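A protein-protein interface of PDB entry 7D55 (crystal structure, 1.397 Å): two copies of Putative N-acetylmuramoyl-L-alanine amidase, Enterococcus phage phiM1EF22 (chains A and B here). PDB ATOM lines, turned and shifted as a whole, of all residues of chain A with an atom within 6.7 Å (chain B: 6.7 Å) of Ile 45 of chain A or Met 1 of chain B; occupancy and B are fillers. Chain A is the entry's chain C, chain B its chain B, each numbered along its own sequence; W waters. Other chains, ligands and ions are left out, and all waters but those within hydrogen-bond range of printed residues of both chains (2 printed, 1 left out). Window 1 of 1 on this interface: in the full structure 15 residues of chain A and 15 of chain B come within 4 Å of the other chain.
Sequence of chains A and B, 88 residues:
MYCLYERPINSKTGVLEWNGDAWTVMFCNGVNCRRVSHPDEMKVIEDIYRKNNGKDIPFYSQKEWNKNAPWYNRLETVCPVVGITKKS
Water W1 lies within hydrogen-bond range of OE1 of Glu 41 of chain A (2.5 Å) and NH1 of Arg 74 of chain B (2.8 Å). Water W2 bridges OD2 of Asp 40 of chain A (2.9 Å) and NE of Arg 74 of chain B (3.1 Å).
Cys 3 of chain A touches none of the printed residues of chain B. Printed residues of chain B within 4 Å of Val 44 of chain A: Arg 74 (3.9 Å) and Leu 75 (3.9 Å). Of chain B, only Met 1 (3.7 Å) and Val 78 (3.9 Å) come within 4 Å of Ile 45 of chain A. Arg 50 of chain A touches none of the printed residues of chain B. Printed residues of chain B within 4 Å of Asn 52 of chain A: Met 1, Tyr 2 and Tyr 49. Of the printed residues of chain A, Tyr 49 of chain B touches Asn 52. The nearest residue of chain B that does not touch Ile 45 of chain A is Leu 75 of chain B (5.7 Å). The nearest residue of chain A that does not touch Met 1 of chain B is Ile 57 of chain A (4.6 Å).
Positions printed for both chains: 2, 3, 27, 28 and 49. Of the 17 pairs that touch across the chains among the printed residues, none has its exchanged pair printed and touching as well.
OH of Tyr 2 of chain A sits at hydrogen-bond distance from N of Met 1 of chain B, at 3.1 Å. The backbone carbonyl oxygen (O) of Tyr 2 of chain B lies within hydrogen-bond range of the side-chain amide nitrogen (ND2) of Asn 52 of chain A, 2.8 Å away. The side-chain hydroxyl (OH) of Tyr 49 of chain B is in hydrogen-bond range of the side-chain amide oxygen (OD1) of Asn 52 of chain A.
Of the 13 printed residues of chain B, 7 touch a printed residue of chain A. Hydrophobic or aromatic side chains of chain B within 4 Å of the printed part of chain A: Met 1, Tyr 2, Tyr 49, Leu 75 and Val 78. Printed residues of chain A that touch a printed residue of chain B: Tyr 2, Phe 27, Asp 40, Glu 41, Val 44, Ile 45, Ile 48, Tyr 49 and Asn 52. Hydrophobic or aromatic side chains of chain A within 4 Å of the printed part of chain B: Tyr 2, Phe 27, Val 44, Ile 45, Ile 48 and Tyr 49. Among the printed residues, no Asp or Glu carboxylate lies within 4 Å of a Lys or Arg side-chain nitrogen of the other chain.
O of Met 1 of chain B sits at hydrogen-bond distance from N of Gly 30 of chain B, at 3.1 Å. The side-chain sulfur (SG) of Cys 28 of chain B is in hydrogen-bond range of the backbone NH (N) of Gly 30 of chain B, 3.4 Å away. The backbone carbonyl oxygen (O) of Gly 30 of chain B lies within hydrogen-bond range of the side-chain sulfur (SG) of Cys 79 of chain B (3.5 Å). ND2 of Asn 52 of chain A is in hydrogen-bond range of O of Ile 48 of chain A, 2.9 Å away. O of Tyr 49 of chain A sits at hydrogen-bond distance from ND2 of Asn 53 of chain A (3.2 Å).
Phe 27 of chain A touches Gly 30 of chain B. Arg 74 of chain B touches Asp 40 of chain A (NE to CB, 3.7 Å). Glu 41 of chain A touches Arg 74 of chain B (CG to O, 3.7 Å). Arg 74 of chain B touches Val 44 of chain A. Val 44 of chain A touches Leu 75 of chain B. CE of Met 1 of chain B touches O of Ile 45 of chain A, at 3.7 Å. Ile 48 of chain A touches Met 1 of chain B. Tyr 2 of chain B touches Ile 48 of chain A (O to CG2, 3.99 Å). Ile 48 of chain A touches Leu 75 of chain B (CD1 to CD1, 3.6 Å). Asn 52 of chain A touches Met 1 of chain B (ND2 to CA, 3.8 Å).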
ATOM      1  N   TYR A   2      -5.189   8.332 -15.787  1.00  0.00           N
ATOM      2  CA  TYR A   2      -4.761   9.591 -16.365  1.00  0.00           C
ATOM      3  C   TYR A   2      -5.796  10.043 -17.374  1.00  0.00           C
ATOM      4  O   TYR A   2      -6.432   9.222 -18.039  1.00  0.00           O
ATOM      5  CB  TYR A   2      -3.435   9.412 -17.103  1.00  0.00           C
ATOM      6  CG  TYR A   2      -2.361   8.890 -16.194  1.00  0.00           C
ATOM      7  CD1 TYR A   2      -1.606   9.759 -15.422  1.00  0.00           C
ATOM      8  CD2 TYR A   2      -2.127   7.529 -16.076  1.00  0.00           C
ATOM      9  CE1 TYR A   2      -0.643   9.293 -14.566  1.00  0.00           C
ATOM     10  CE2 TYR A   2      -1.162   7.052 -15.221  1.00  0.00           C
ATOM     11  CZ  TYR A   2      -0.423   7.940 -14.471  1.00  0.00           C
ATOM     12  OH  TYR A   2       0.544   7.474 -13.613  1.00  0.00           O
ATOM     13  N   CYS A   3      -5.960  11.354 -17.496  1.00  0.00           N
ATOM     14  CA  CYS A   3      -6.743  11.856 -18.615  1.00  0.00           C
ATOM     15  C   CYS A   3      -6.437  13.327 -18.824  1.00  0.00           C
ATOM     16  O   CYS A   3      -5.866  14.000 -17.960  1.00  0.00           O
ATOM     17  CB  CYS A   3      -8.245  11.634 -18.407  1.00  0.00           C
ATOM     18  SG  CYS A   3      -8.962  12.573 -17.044  1.00  0.00           S
ATOM     19  N   LEU A   4      -6.811  13.808 -20.000  1.00  0.00           N
ATOM     20  CA  LEU A   4      -6.855  15.228 -20.297  1.00  0.00           C
ATOM     21  C   LEU A   4      -8.314  15.603 -20.493  1.00  0.00           C
ATOM     22  O   LEU A   4      -9.113  14.804 -20.994  1.00  0.00           O
ATOM     23  CB  LEU A   4      -6.069  15.544 -21.568  1.00  0.00           C
ATOM     24  CG  LEU A   4      -4.561  15.326 -21.455  1.00  0.00           C
ATOM     25  CD1 LEU A   4      -3.905  15.250 -22.832  1.00  0.00           C
ATOM     26  CD2 LEU A   4      -3.952  16.450 -20.632  1.00  0.00           C
ATOM     27  N   MET A  26      -6.807  20.548 -18.808  1.00  0.00           N
ATOM     28  CA  MET A  26      -6.320  20.123 -17.507  1.00  0.00           C
ATOM     29  C   MET A  26      -5.836  18.690 -17.624  1.00  0.00           C
ATOM     30  O   MET A  26      -6.297  17.932 -18.482  1.00  0.00           O
ATOM     31  CB  MET A  26      -7.431  20.108 -16.440  1.00  0.00           C
ATOM     32  CG  MET A  26      -8.179  21.398 -16.273  1.00  0.00           C
ATOM     33  SD  MET A  26      -7.308  22.610 -15.257  1.00  0.00           S
ATOM     34  CE  MET A  26      -7.257  21.799 -13.649  1.00  0.00           C
ATOM     35  N   PHE A  27      -4.919  18.319 -16.735  1.00  0.00           N
ATOM     36  CA  PHE A  27      -4.338  16.985 -16.702  1.00  0.00           C
ATOM     37  C   PHE A  27      -4.630  16.371 -15.344  1.00  0.00           C
ATOM     38  O   PHE A  27      -4.355  16.988 -14.307  1.00  0.00           O
ATOM     39  CB  PHE A  27      -2.828  17.073 -16.922  1.00  0.00           C
ATOM     40  CG  PHE A  27      -2.077  15.804 -16.635  1.00  0.00           C
ATOM     41  CD1 PHE A  27      -2.334  14.642 -17.346  1.00  0.00           C
ATOM     42  CD2 PHE A  27      -1.081  15.796 -15.685  1.00  0.00           C
ATOM     43  CE1 PHE A  27      -1.613  13.476 -17.095  1.00  0.00           C
ATOM     44  CE2 PHE A  27      -0.361  14.638 -15.429  1.00  0.00           C
ATOM     45  CZ  PHE A  27      -0.630  13.478 -16.137  1.00  0.00           C
ATOM     46  N   CYS A  28      -5.191  15.170 -15.347  1.00  0.00           N
ATOM     47  CA  CYS A  28      -5.465  14.431 -14.125  1.00  0.00           C
ATOM     48  C   CYS A  28      -4.559  13.212 -14.087  1.00  0.00           C
ATOM     49  O   CYS A  28      -4.441  12.495 -15.083  1.00  0.00           O
ATOM     50  CB  CYS A  28      -6.926  13.977 -14.085  1.00  0.00           C
ATOM     51  SG  CYS A  28      -7.295  12.974 -12.638  1.00  0.00           S
ATOM     52  N   VAL A  36      -3.105  22.683 -17.856  1.00  0.00           N
ATOM     53  CA  VAL A  36      -2.200  22.567 -18.997  1.00  0.00           C
ATOM     54  C   VAL A  36      -2.345  23.865 -19.785  1.00  0.00           C
ATOM     55  O   VAL A  36      -3.405  24.124 -20.369  1.00  0.00           O
ATOM     56  CB  VAL A  36      -2.564  21.349 -19.858  1.00  0.00           C
ATOM     57  CG1 VAL A  36      -1.724  21.295 -21.142  1.00  0.00           C
ATOM     58  CG2 VAL A  36      -2.455  20.054 -19.038  1.00  0.00           C
ATOM     59  N   ASP A  40       2.322  22.510 -26.114  1.00  0.00           N
ATOM     60  CA  ASP A  40       3.478  21.627 -25.986  1.00  0.00           C
ATOM     61  C   ASP A  40       3.491  20.893 -24.654  1.00  0.00           C
ATOM     62  O   ASP A  40       4.113  19.825 -24.548  1.00  0.00           O
ATOM     63  CB  ASP A  40       4.778  22.397 -26.217  1.00  0.00           C
ATOM     64  CG  ASP A  40       5.001  22.747 -27.688  1.00  0.00           C
ATOM     65  OD1 ASP A  40       4.173  22.321 -28.524  1.00  0.00           O
ATOM     66  OD2 ASP A  40       5.995  23.443 -28.006  1.00  0.00           O
ATOM     67  N   GLU A  41       2.846  21.446 -23.616  1.00  0.00           N
ATOM     68  CA  GLU A  41       2.623  20.656 -22.407  1.00  0.00           C
ATOM     69  C   GLU A  41       1.682  19.500 -22.701  1.00  0.00           C
ATOM     70  O   GLU A  41       1.899  18.374 -22.240  1.00  0.00           O
ATOM     71  CB  GLU A  41       2.031  21.522 -21.291  1.00  0.00           C
ATOM     72  CG  GLU A  41       3.011  22.500 -20.653  1.00  0.00           C
ATOM     73  CD  GLU A  41       2.308  23.659 -19.952  1.00  0.00           C
ATOM     74  OE1 GLU A  41       2.928  24.738 -19.811  1.00  0.00           O
ATOM     75  OE2 GLU A  41       1.138  23.492 -19.540  1.00  0.00           O
ATOM     76  N   MET A  42       0.633  19.762 -23.477  1.00  0.00           N
ATOM     77  CA  MET A  42      -0.281  18.693 -23.850  1.00  0.00           C
ATOM     78  C   MET A  42       0.442  17.639 -24.681  1.00  0.00           C
ATOM     79  O   MET A  42       0.279  16.432 -24.457  1.00  0.00           O
ATOM     80  CB  MET A  42      -1.479  19.279 -24.598  1.00  0.00           C
ATOM     81  CG  MET A  42      -2.609  18.309 -24.763  1.00  0.00           C
ATOM     82  SD  MET A  42      -4.032  19.115 -25.516  1.00  0.00           S
ATOM     83  CE  MET A  42      -5.176  17.737 -25.601  1.00  0.00           C
ATOM     84  N   LYS A  43       1.298  18.077 -25.603  1.00  0.00           N
ATOM     85  CA  LYS A  43       1.998  17.129 -26.461  1.00  0.00           C
ATOM     86  C   LYS A  43       2.943  16.243 -25.656  1.00  0.00           C
ATOM     87  O   LYS A  43       3.046  15.039 -25.920  1.00  0.00           O
ATOM     88  CB  LYS A  43       2.758  17.871 -27.565  1.00  0.00           C
ATOM     89  CG  LYS A  43       2.995  17.016 -28.798  1.00  0.00           C
ATOM     90  CD  LYS A  43       3.599  17.801 -29.962  1.00  0.00           C
ATOM     91  CE  LYS A  43       4.408  16.880 -30.883  1.00  0.00           C
ATOM     92  NZ  LYS A  43       5.868  17.212 -30.956  1.00  0.00           N
ATOM     93  N   VAL A  44       3.643  16.811 -24.672  1.00  0.00           N
ATOM     94  CA  VAL A  44       4.587  15.997 -23.912  1.00  0.00           C
ATOM     95  C   VAL A  44       3.849  14.977 -23.047  1.00  0.00           C
ATOM     96  O   VAL A  44       4.291  13.830 -22.906  1.00  0.00           O
ATOM     97  CB  VAL A  44       5.602  16.866 -23.142  1.00  0.00           C
ATOM     98  CG1 VAL A  44       5.030  17.414 -21.869  1.00  0.00           C
ATOM     99  CG2 VAL A  44       6.865  16.073 -22.856  1.00  0.00           C
ATOM    100  N   ILE A  45       2.693  15.360 -22.495  1.00  0.00           N
ATOM    101  CA  ILE A  45       1.872  14.425 -21.725  1.00  0.00           C
ATOM    102  C   ILE A  45       1.399  13.287 -22.618  1.00  0.00           C
ATOM    103  O   ILE A  45       1.485  12.105 -22.255  1.00  0.00           O
ATOM    104  CB  ILE A  45       0.679  15.160 -21.091  1.00  0.00           C
ATOM    105  CG1 ILE A  45       1.143  16.055 -19.953  1.00  0.00           C
ATOM    106  CG2 ILE A  45      -0.373  14.159 -20.628  1.00  0.00           C
ATOM    107  CD1 ILE A  45       0.084  17.033 -19.490  1.00  0.00           C
ATOM    108  N   GLU A  46       0.892  13.632 -23.805  1.00  0.00           N
ATOM    109  CA  GLU A  46       0.430  12.612 -24.737  1.00  0.00           C
ATOM    110  C   GLU A  46       1.559  11.670 -25.128  1.00  0.00           C
ATOM    111  O   GLU A  46       1.356  10.453 -25.231  1.00  0.00           O
ATOM    112  CB  GLU A  46      -0.155  13.279 -25.978  1.00  0.00           C
ATOM    113  CG  GLU A  46      -1.438  14.033 -25.715  1.00  0.00           C
ATOM    114  CD  GLU A  46      -1.821  14.954 -26.861  1.00  0.00           C
ATOM    115  OE1 GLU A  46      -0.972  15.197 -27.752  1.00  0.00           O
ATOM    116  OE2 GLU A  46      -2.965  15.451 -26.866  1.00  0.00           O
ATOM    117  N   ASP A  47       2.759  12.213 -25.342  1.00  0.00           N
ATOM    118  CA  ASP A  47       3.884  11.393 -25.776  1.00  0.00           C
ATOM    119  C   ASP A  47       4.318  10.427 -24.680  1.00  0.00           C
ATOM    120  O   ASP A  47       4.536   9.238 -24.937  1.00  0.00           O
ATOM    121  CB  ASP A  47       5.053  12.288 -26.186  1.00  0.00           C
ATOM    122  CG  ASP A  47       6.119  11.530 -26.927  1.00  0.00           C
ATOM    123  OD1 ASP A  47       5.822  11.027 -28.032  1.00  0.00           O
ATOM    124  OD2 ASP A  47       7.245  11.434 -26.410  1.00  0.00           O
ATOM    125  N   ILE A  48       4.459  10.925 -23.450  1.00  0.00           N
ATOM    126  CA  ILE A  48       4.863  10.064 -22.336  1.00  0.00           C
ATOM    127  C   ILE A  48       3.822   8.978 -22.095  1.00  0.00           C
ATOM    128  O   ILE A  48       4.165   7.808 -21.867  1.00  0.00           O
ATOM    129  CB  ILE A  48       5.125  10.910 -21.076  1.00  0.00           C
ATOM    130  CG1 ILE A  48       6.330  11.824 -21.296  1.00  0.00           C
ATOM    131  CG2 ILE A  48       5.377  10.022 -19.854  1.00  0.00           C
ATOM    132  CD1 ILE A  48       6.387  12.956 -20.285  1.00  0.00           C
ATOM    133  N   TYR A  49       2.538   9.342 -22.118  1.00  0.00           N
ATOM    134  CA  TYR A  49       1.499   8.338 -21.914  1.00  0.00           C
ATOM    135  C   TYR A  49       1.603   7.236 -22.959  1.00  0.00           C
ATOM    136  O   TYR A  49       1.556   6.045 -22.628  1.00  0.00           O
ATOM    137  CB  TYR A  49       0.108   8.979 -21.935  1.00  0.00           C
ATOM    138  CG  TYR A  49      -0.995   7.996 -21.592  1.00  0.00           C
ATOM    139  CD1 TYR A  49      -1.504   7.133 -22.555  1.00  0.00           C
ATOM    140  CD2 TYR A  49      -1.536   7.934 -20.306  1.00  0.00           C
ATOM    141  CE1 TYR A  49      -2.518   6.236 -22.254  1.00  0.00           C
ATOM    142  CE2 TYR A  49      -2.553   7.039 -19.998  1.00  0.00           C
ATOM    143  CZ  TYR A  49      -3.033   6.192 -20.979  1.00  0.00           C
ATOM    144  OH  TYR A  49      -4.028   5.303 -20.691  1.00  0.00           O
ATOM    145  N   ARG A  50       1.765   7.618 -24.228  1.00  0.00           N
ATOM    146  CA  ARG A  50       1.860   6.634 -25.304  1.00  0.00           C
ATOM    147  C   ARG A  50       3.103   5.756 -25.161  1.00  0.00           C
ATOM    148  O   ARG A  50       3.048   4.546 -25.408  1.00  0.00           O
ATOM    149  CB  ARG A  50       1.854   7.352 -26.654  1.00  0.00           C
ATOM    150  CG  ARG A  50       1.266   6.545 -27.782  1.00  0.00           C
ATOM    151  CD  ARG A  50       0.867   7.443 -28.958  1.00  0.00           C
ATOM    152  NE  ARG A  50       1.562   8.730 -28.938  1.00  0.00           N
ATOM    153  CZ  ARG A  50       0.961   9.919 -28.979  1.00  0.00           C
ATOM    154  NH1 ARG A  50      -0.363   9.998 -29.049  1.00  0.00           N
ATOM    155  NH2 ARG A  50       1.685  11.033 -28.956  1.00  0.00           N
ATOM    156  N   ASN A  52       4.455   4.844 -22.452  1.00  0.00           N
ATOM    157  CA  ASN A  52       4.236   3.911 -21.349  1.00  0.00           C
ATOM    158  C   ASN A  52       3.195   2.860 -21.702  1.00  0.00           C
ATOM    159  O   ASN A  52       3.325   1.695 -21.314  1.00  0.00           O
ATOM    160  CB  ASN A  52       3.752   4.664 -20.110  1.00  0.00           C
ATOM    161  CG  ASN A  52       4.894   5.216 -19.276  1.00  0.00           C
ATOM    162  OD1 ASN A  52       5.410   4.541 -18.387  1.00  0.00           O
ATOM    163  ND2 ASN A  52       5.282   6.448 -19.549  1.00  0.00           N
ATOM    164  N   ASN A  53       2.152   3.251 -22.430  1.00  0.00           N
ATOM    165  CA  ASN A  53       0.952   2.441 -22.517  1.00  0.00           C
ATOM    166  C   ASN A  53       0.585   1.977 -23.918  1.00  0.00           C
ATOM    167  O   ASN A  53      -0.295   1.119 -24.050  1.00  0.00           O
ATOM    168  CB  ASN A  53      -0.221   3.186 -21.863  1.00  0.00           C
ATOM    169  CG  ASN A  53       0.075   3.537 -20.418  1.00  0.00           C
ATOM    170  OD1 ASN A  53       0.403   2.655 -19.618  1.00  0.00           O
ATOM    171  ND2 ASN A  53       0.010   4.820 -20.082  1.00  0.00           N
ATOM    172  N   ILE A  57      -3.666   8.838 -24.577  1.00  0.00           N
ATOM    173  CA  ILE A  57      -4.236   9.178 -23.267  1.00  0.00           C
ATOM    174  C   ILE A  57      -5.719   9.487 -23.423  1.00  0.00           C
ATOM    175  O   ILE A  57      -6.118  10.103 -24.432  1.00  0.00           O
ATOM    176  CB  ILE A  57      -3.484  10.368 -22.641  1.00  0.00           C
ATOM    177  CG1 ILE A  57      -3.925  10.581 -21.190  1.00  0.00           C
ATOM    178  CG2 ILE A  57      -3.648  11.652 -23.474  1.00  0.00           C
ATOM    179  CD1 ILE A  57      -3.054  11.566 -20.436  1.00  0.00           C
ATOM    180  N   MET B   1       2.261   6.724 -16.084  1.00  0.00           N
ATOM    181  CA  MET B   1       3.161   7.698 -16.699  1.00  0.00           C
ATOM    182  C   MET B   1       4.455   7.903 -15.927  1.00  0.00           C
ATOM    183  O   MET B   1       4.503   8.596 -14.915  1.00  0.00           O
ATOM    184  CB  MET B   1       2.467   9.032 -16.897  1.00  0.00           C
ATOM    185  CG  MET B   1       1.764   9.082 -18.214  1.00  0.00           C
ATOM    186  SD  MET B   1       0.932  10.634 -18.409  1.00  0.00           S
ATOM    187  CE  MET B   1       2.304  11.752 -18.648  1.00  0.00           C
ATOM    188  N   TYR B   2       5.501   7.277 -16.426  1.00  0.00           N
ATOM    189  CA  TYR B   2       6.822   7.374 -15.847  1.00  0.00           C
ATOM    190  C   TYR B   2       7.807   7.636 -16.970  1.00  0.00           C
ATOM    191  O   TYR B   2       7.597   7.206 -18.110  1.00  0.00           O
ATOM    192  CB  TYR B   2       7.188   6.054 -15.157  1.00  0.00           C
ATOM    193  CG  TYR B   2       6.194   5.683 -14.099  1.00  0.00           C
ATOM    194  CD1 TYR B   2       6.334   6.142 -12.795  1.00  0.00           C
ATOM    195  CD2 TYR B   2       5.088   4.894 -14.405  1.00  0.00           C
ATOM    196  CE1 TYR B   2       5.397   5.827 -11.818  1.00  0.00           C
ATOM    197  CE2 TYR B   2       4.151   4.566 -13.437  1.00  0.00           C
ATOM    198  CZ  TYR B   2       4.312   5.031 -12.145  1.00  0.00           C
ATOM    199  OH  TYR B   2       3.373   4.695 -11.186  1.00  0.00           O
ATOM    200  N   CYS B   3       8.872   8.360 -16.649  1.00  0.00           N
ATOM    201  CA  CYS B   3       9.979   8.447 -17.592  1.00  0.00           C
ATOM    202  C   CYS B   3      11.240   8.866 -16.863  1.00  0.00           C
ATOM    203  O   CYS B   3      11.197   9.383 -15.742  1.00  0.00           O
ATOM    204  CB  CYS B   3       9.674   9.379 -18.775  1.00  0.00           C
ATOM    205  SG  CYS B   3       9.474  11.110 -18.338  1.00  0.00           S
ATOM    206  N   PHE B  27      13.681  11.824 -12.768  1.00  0.00           N
ATOM    207  CA  PHE B  27      12.681  10.765 -12.773  1.00  0.00           C
ATOM    208  C   PHE B  27      11.319  11.424 -12.624  1.00  0.00           C
ATOM    209  O   PHE B  27      11.095  12.179 -11.673  1.00  0.00           O
ATOM    210  CB  PHE B  27      12.924   9.808 -11.599  1.00  0.00           C
ATOM    211  CG  PHE B  27      11.774   8.892 -11.308  1.00  0.00           C
ATOM    212  CD1 PHE B  27      11.267   8.060 -12.292  1.00  0.00           C
ATOM    213  CD2 PHE B  27      11.216   8.848 -10.039  1.00  0.00           C
ATOM    214  CE1 PHE B  27      10.218   7.195 -12.015  1.00  0.00           C
ATOM    215  CE2 PHE B  27      10.159   7.987  -9.755  1.00  0.00           C
ATOM    216  CZ  PHE B  27       9.664   7.162 -10.738  1.00  0.00           C
ATOM    217  N   CYS B  28      10.418  11.151 -13.562  1.00  0.00           N
ATOM    218  CA  CYS B  28       9.045  11.631 -13.492  1.00  0.00           C
ATOM    219  C   CYS B  28       8.115  10.460 -13.200  1.00  0.00           C
ATOM    220  O   CYS B  28       8.206   9.417 -13.853  1.00  0.00           O
ATOM    221  CB  CYS B  28       8.635  12.281 -14.809  1.00  0.00           C
ATOM    222  SG  CYS B  28       6.926  12.844 -14.815  1.00  0.00           S
ATOM    223  N   ASN B  29       7.213  10.637 -12.232  1.00  0.00           N
ATOM    224  CA  ASN B  29       6.243   9.604 -11.876  1.00  0.00           C
ATOM    225  C   ASN B  29       4.809  10.018 -12.180  1.00  0.00           C
ATOM    226  O   ASN B  29       3.869   9.439 -11.625  1.00  0.00           O
ATOM    227  CB  ASN B  29       6.387   9.221 -10.400  1.00  0.00           C
ATOM    228  CG  ASN B  29       6.219  10.413  -9.486  1.00  0.00           C
ATOM    229  OD1 ASN B  29       5.742  11.457  -9.920  1.00  0.00           O
ATOM    230  ND2 ASN B  29       6.614  10.272  -8.221  1.00  0.00           N
ATOM    231  N   GLY B  30       4.618  11.012 -13.052  1.00  0.00           N
ATOM    232  CA  GLY B  30       3.293  11.530 -13.320  1.00  0.00           C
ATOM    233  C   GLY B  30       2.779  12.509 -12.290  1.00  0.00           C
ATOM    234  O   GLY B  30       1.763  13.169 -12.539  1.00  0.00           O
ATOM    235  N   VAL B  31       3.446  12.623 -11.147  1.00  0.00           N
ATOM    236  CA  VAL B  31       3.081  13.554 -10.093  1.00  0.00           C
ATOM    237  C   VAL B  31       4.123  14.655  -9.953  1.00  0.00           C
ATOM    238  O   VAL B  31       3.795  15.839  -9.913  1.00  0.00           O
ATOM    239  CB  VAL B  31       2.879  12.808  -8.757  1.00  0.00           C
ATOM    240  CG1 VAL B  31       2.494  13.776  -7.652  1.00  0.00           C
ATOM    241  CG2 VAL B  31       1.862  11.683  -8.927  1.00  0.00           C
ATOM    242  N   TYR B  49      10.390  -0.661 -12.582  1.00  0.00           N
ATOM    243  CA  TYR B  49       9.500  -0.459 -13.718  1.00  0.00           C
ATOM    244  C   TYR B  49       9.366  -1.736 -14.537  1.00  0.00           C
ATOM    245  O   TYR B  49       8.254  -2.145 -14.893  1.00  0.00           O
ATOM    246  CB  TYR B  49       9.987   0.699 -14.592  1.00  0.00           C
ATOM    247  CG  TYR B  49       9.007   1.039 -15.691  1.00  0.00           C
ATOM    248  CD1 TYR B  49       8.973   0.302 -16.878  1.00  0.00           C
ATOM    249  CD2 TYR B  49       8.111   2.097 -15.552  1.00  0.00           C
ATOM    250  CE1 TYR B  49       8.085   0.608 -17.884  1.00  0.00           C
ATOM    251  CE2 TYR B  49       7.220   2.406 -16.551  1.00  0.00           C
ATOM    252  CZ  TYR B  49       7.212   1.665 -17.715  1.00  0.00           C
ATOM    253  OH  TYR B  49       6.334   1.982 -18.715  1.00  0.00           O
ATOM    254  N   ARG B  74       8.375  21.765 -20.423  1.00  0.00           N
ATOM    255  CA  ARG B  74       6.946  21.491 -20.489  1.00  0.00           C
ATOM    256  C   ARG B  74       6.553  20.432 -19.471  1.00  0.00           C
ATOM    257  O   ARG B  74       5.562  20.587 -18.749  1.00  0.00           O
ATOM    258  CB  ARG B  74       6.578  21.031 -21.899  1.00  0.00           C
ATOM    259  CG  ARG B  74       7.056  21.963 -22.989  1.00  0.00           C
ATOM    260  CD  ARG B  74       6.515  23.359 -22.774  1.00  0.00           C
ATOM    261  NE  ARG B  74       6.895  24.253 -23.860  1.00  0.00           N
ATOM    262  CZ  ARG B  74       6.521  25.525 -23.947  1.00  0.00           C
ATOM    263  NH1 ARG B  74       5.748  26.054 -23.006  1.00  0.00           N
ATOM    264  NH2 ARG B  74       6.907  26.263 -24.981  1.00  0.00           N
ATOM    265  N   LEU B  75       7.318  19.340 -19.401  1.00  0.00           N
ATOM    266  CA  LEU B  75       7.002  18.276 -18.452  1.00  0.00           C
ATOM    267  C   LEU B  75       7.026  18.797 -17.020  1.00  0.00           C
ATOM    268  O   LEU B  75       6.120  18.510 -16.221  1.00  0.00           O
ATOM    269  CB  LEU B  75       7.972  17.106 -18.626  1.00  0.00           C
ATOM    270  CG  LEU B  75       7.793  15.988 -17.606  1.00  0.00           C
ATOM    271  CD1 LEU B  75       6.367  15.478 -17.666  1.00  0.00           C
ATOM    272  CD2 LEU B  75       8.767  14.854 -17.852  1.00  0.00           C
ATOM    273  N   VAL B  78       3.883  20.614 -15.816  1.00  0.00           N
ATOM    274  CA  VAL B  78       2.722  19.804 -15.472  1.00  0.00           C
ATOM    275  C   VAL B  78       2.998  18.814 -14.344  1.00  0.00           C
ATOM    276  O   VAL B  78       2.050  18.392 -13.661  1.00  0.00           O
ATOM    277  CB  VAL B  78       2.153  19.095 -16.711  1.00  0.00           C
ATOM    278  CG1 VAL B  78       1.822  20.109 -17.789  1.00  0.00           C
ATOM    279  CG2 VAL B  78       3.126  18.070 -17.228  1.00  0.00           C
ATOM    280  N   CYS B  79       4.262  18.428 -14.137  1.00  0.00           N
ATOM    281  CA  CYS B  79       4.674  17.559 -13.033  1.00  0.00           C
ATOM    282  C   CYS B  79       5.823  18.273 -12.334  1.00  0.00           C
ATOM    283  O   CYS B  79       6.994  18.046 -12.660  1.00  0.00           O
ATOM    284  CB  CYS B  79       5.121  16.194 -13.547  1.00  0.00           C
ATOM    285  SG  CYS B  79       3.842  15.259 -14.394  1.00  0.00           S
HETATM  286  O   HOH W   1       5.255  25.417 -20.331  1.00  0.00           O
HETATM  287  O   HOH W   2       8.399  23.448 -26.400  1.00  0.00           O
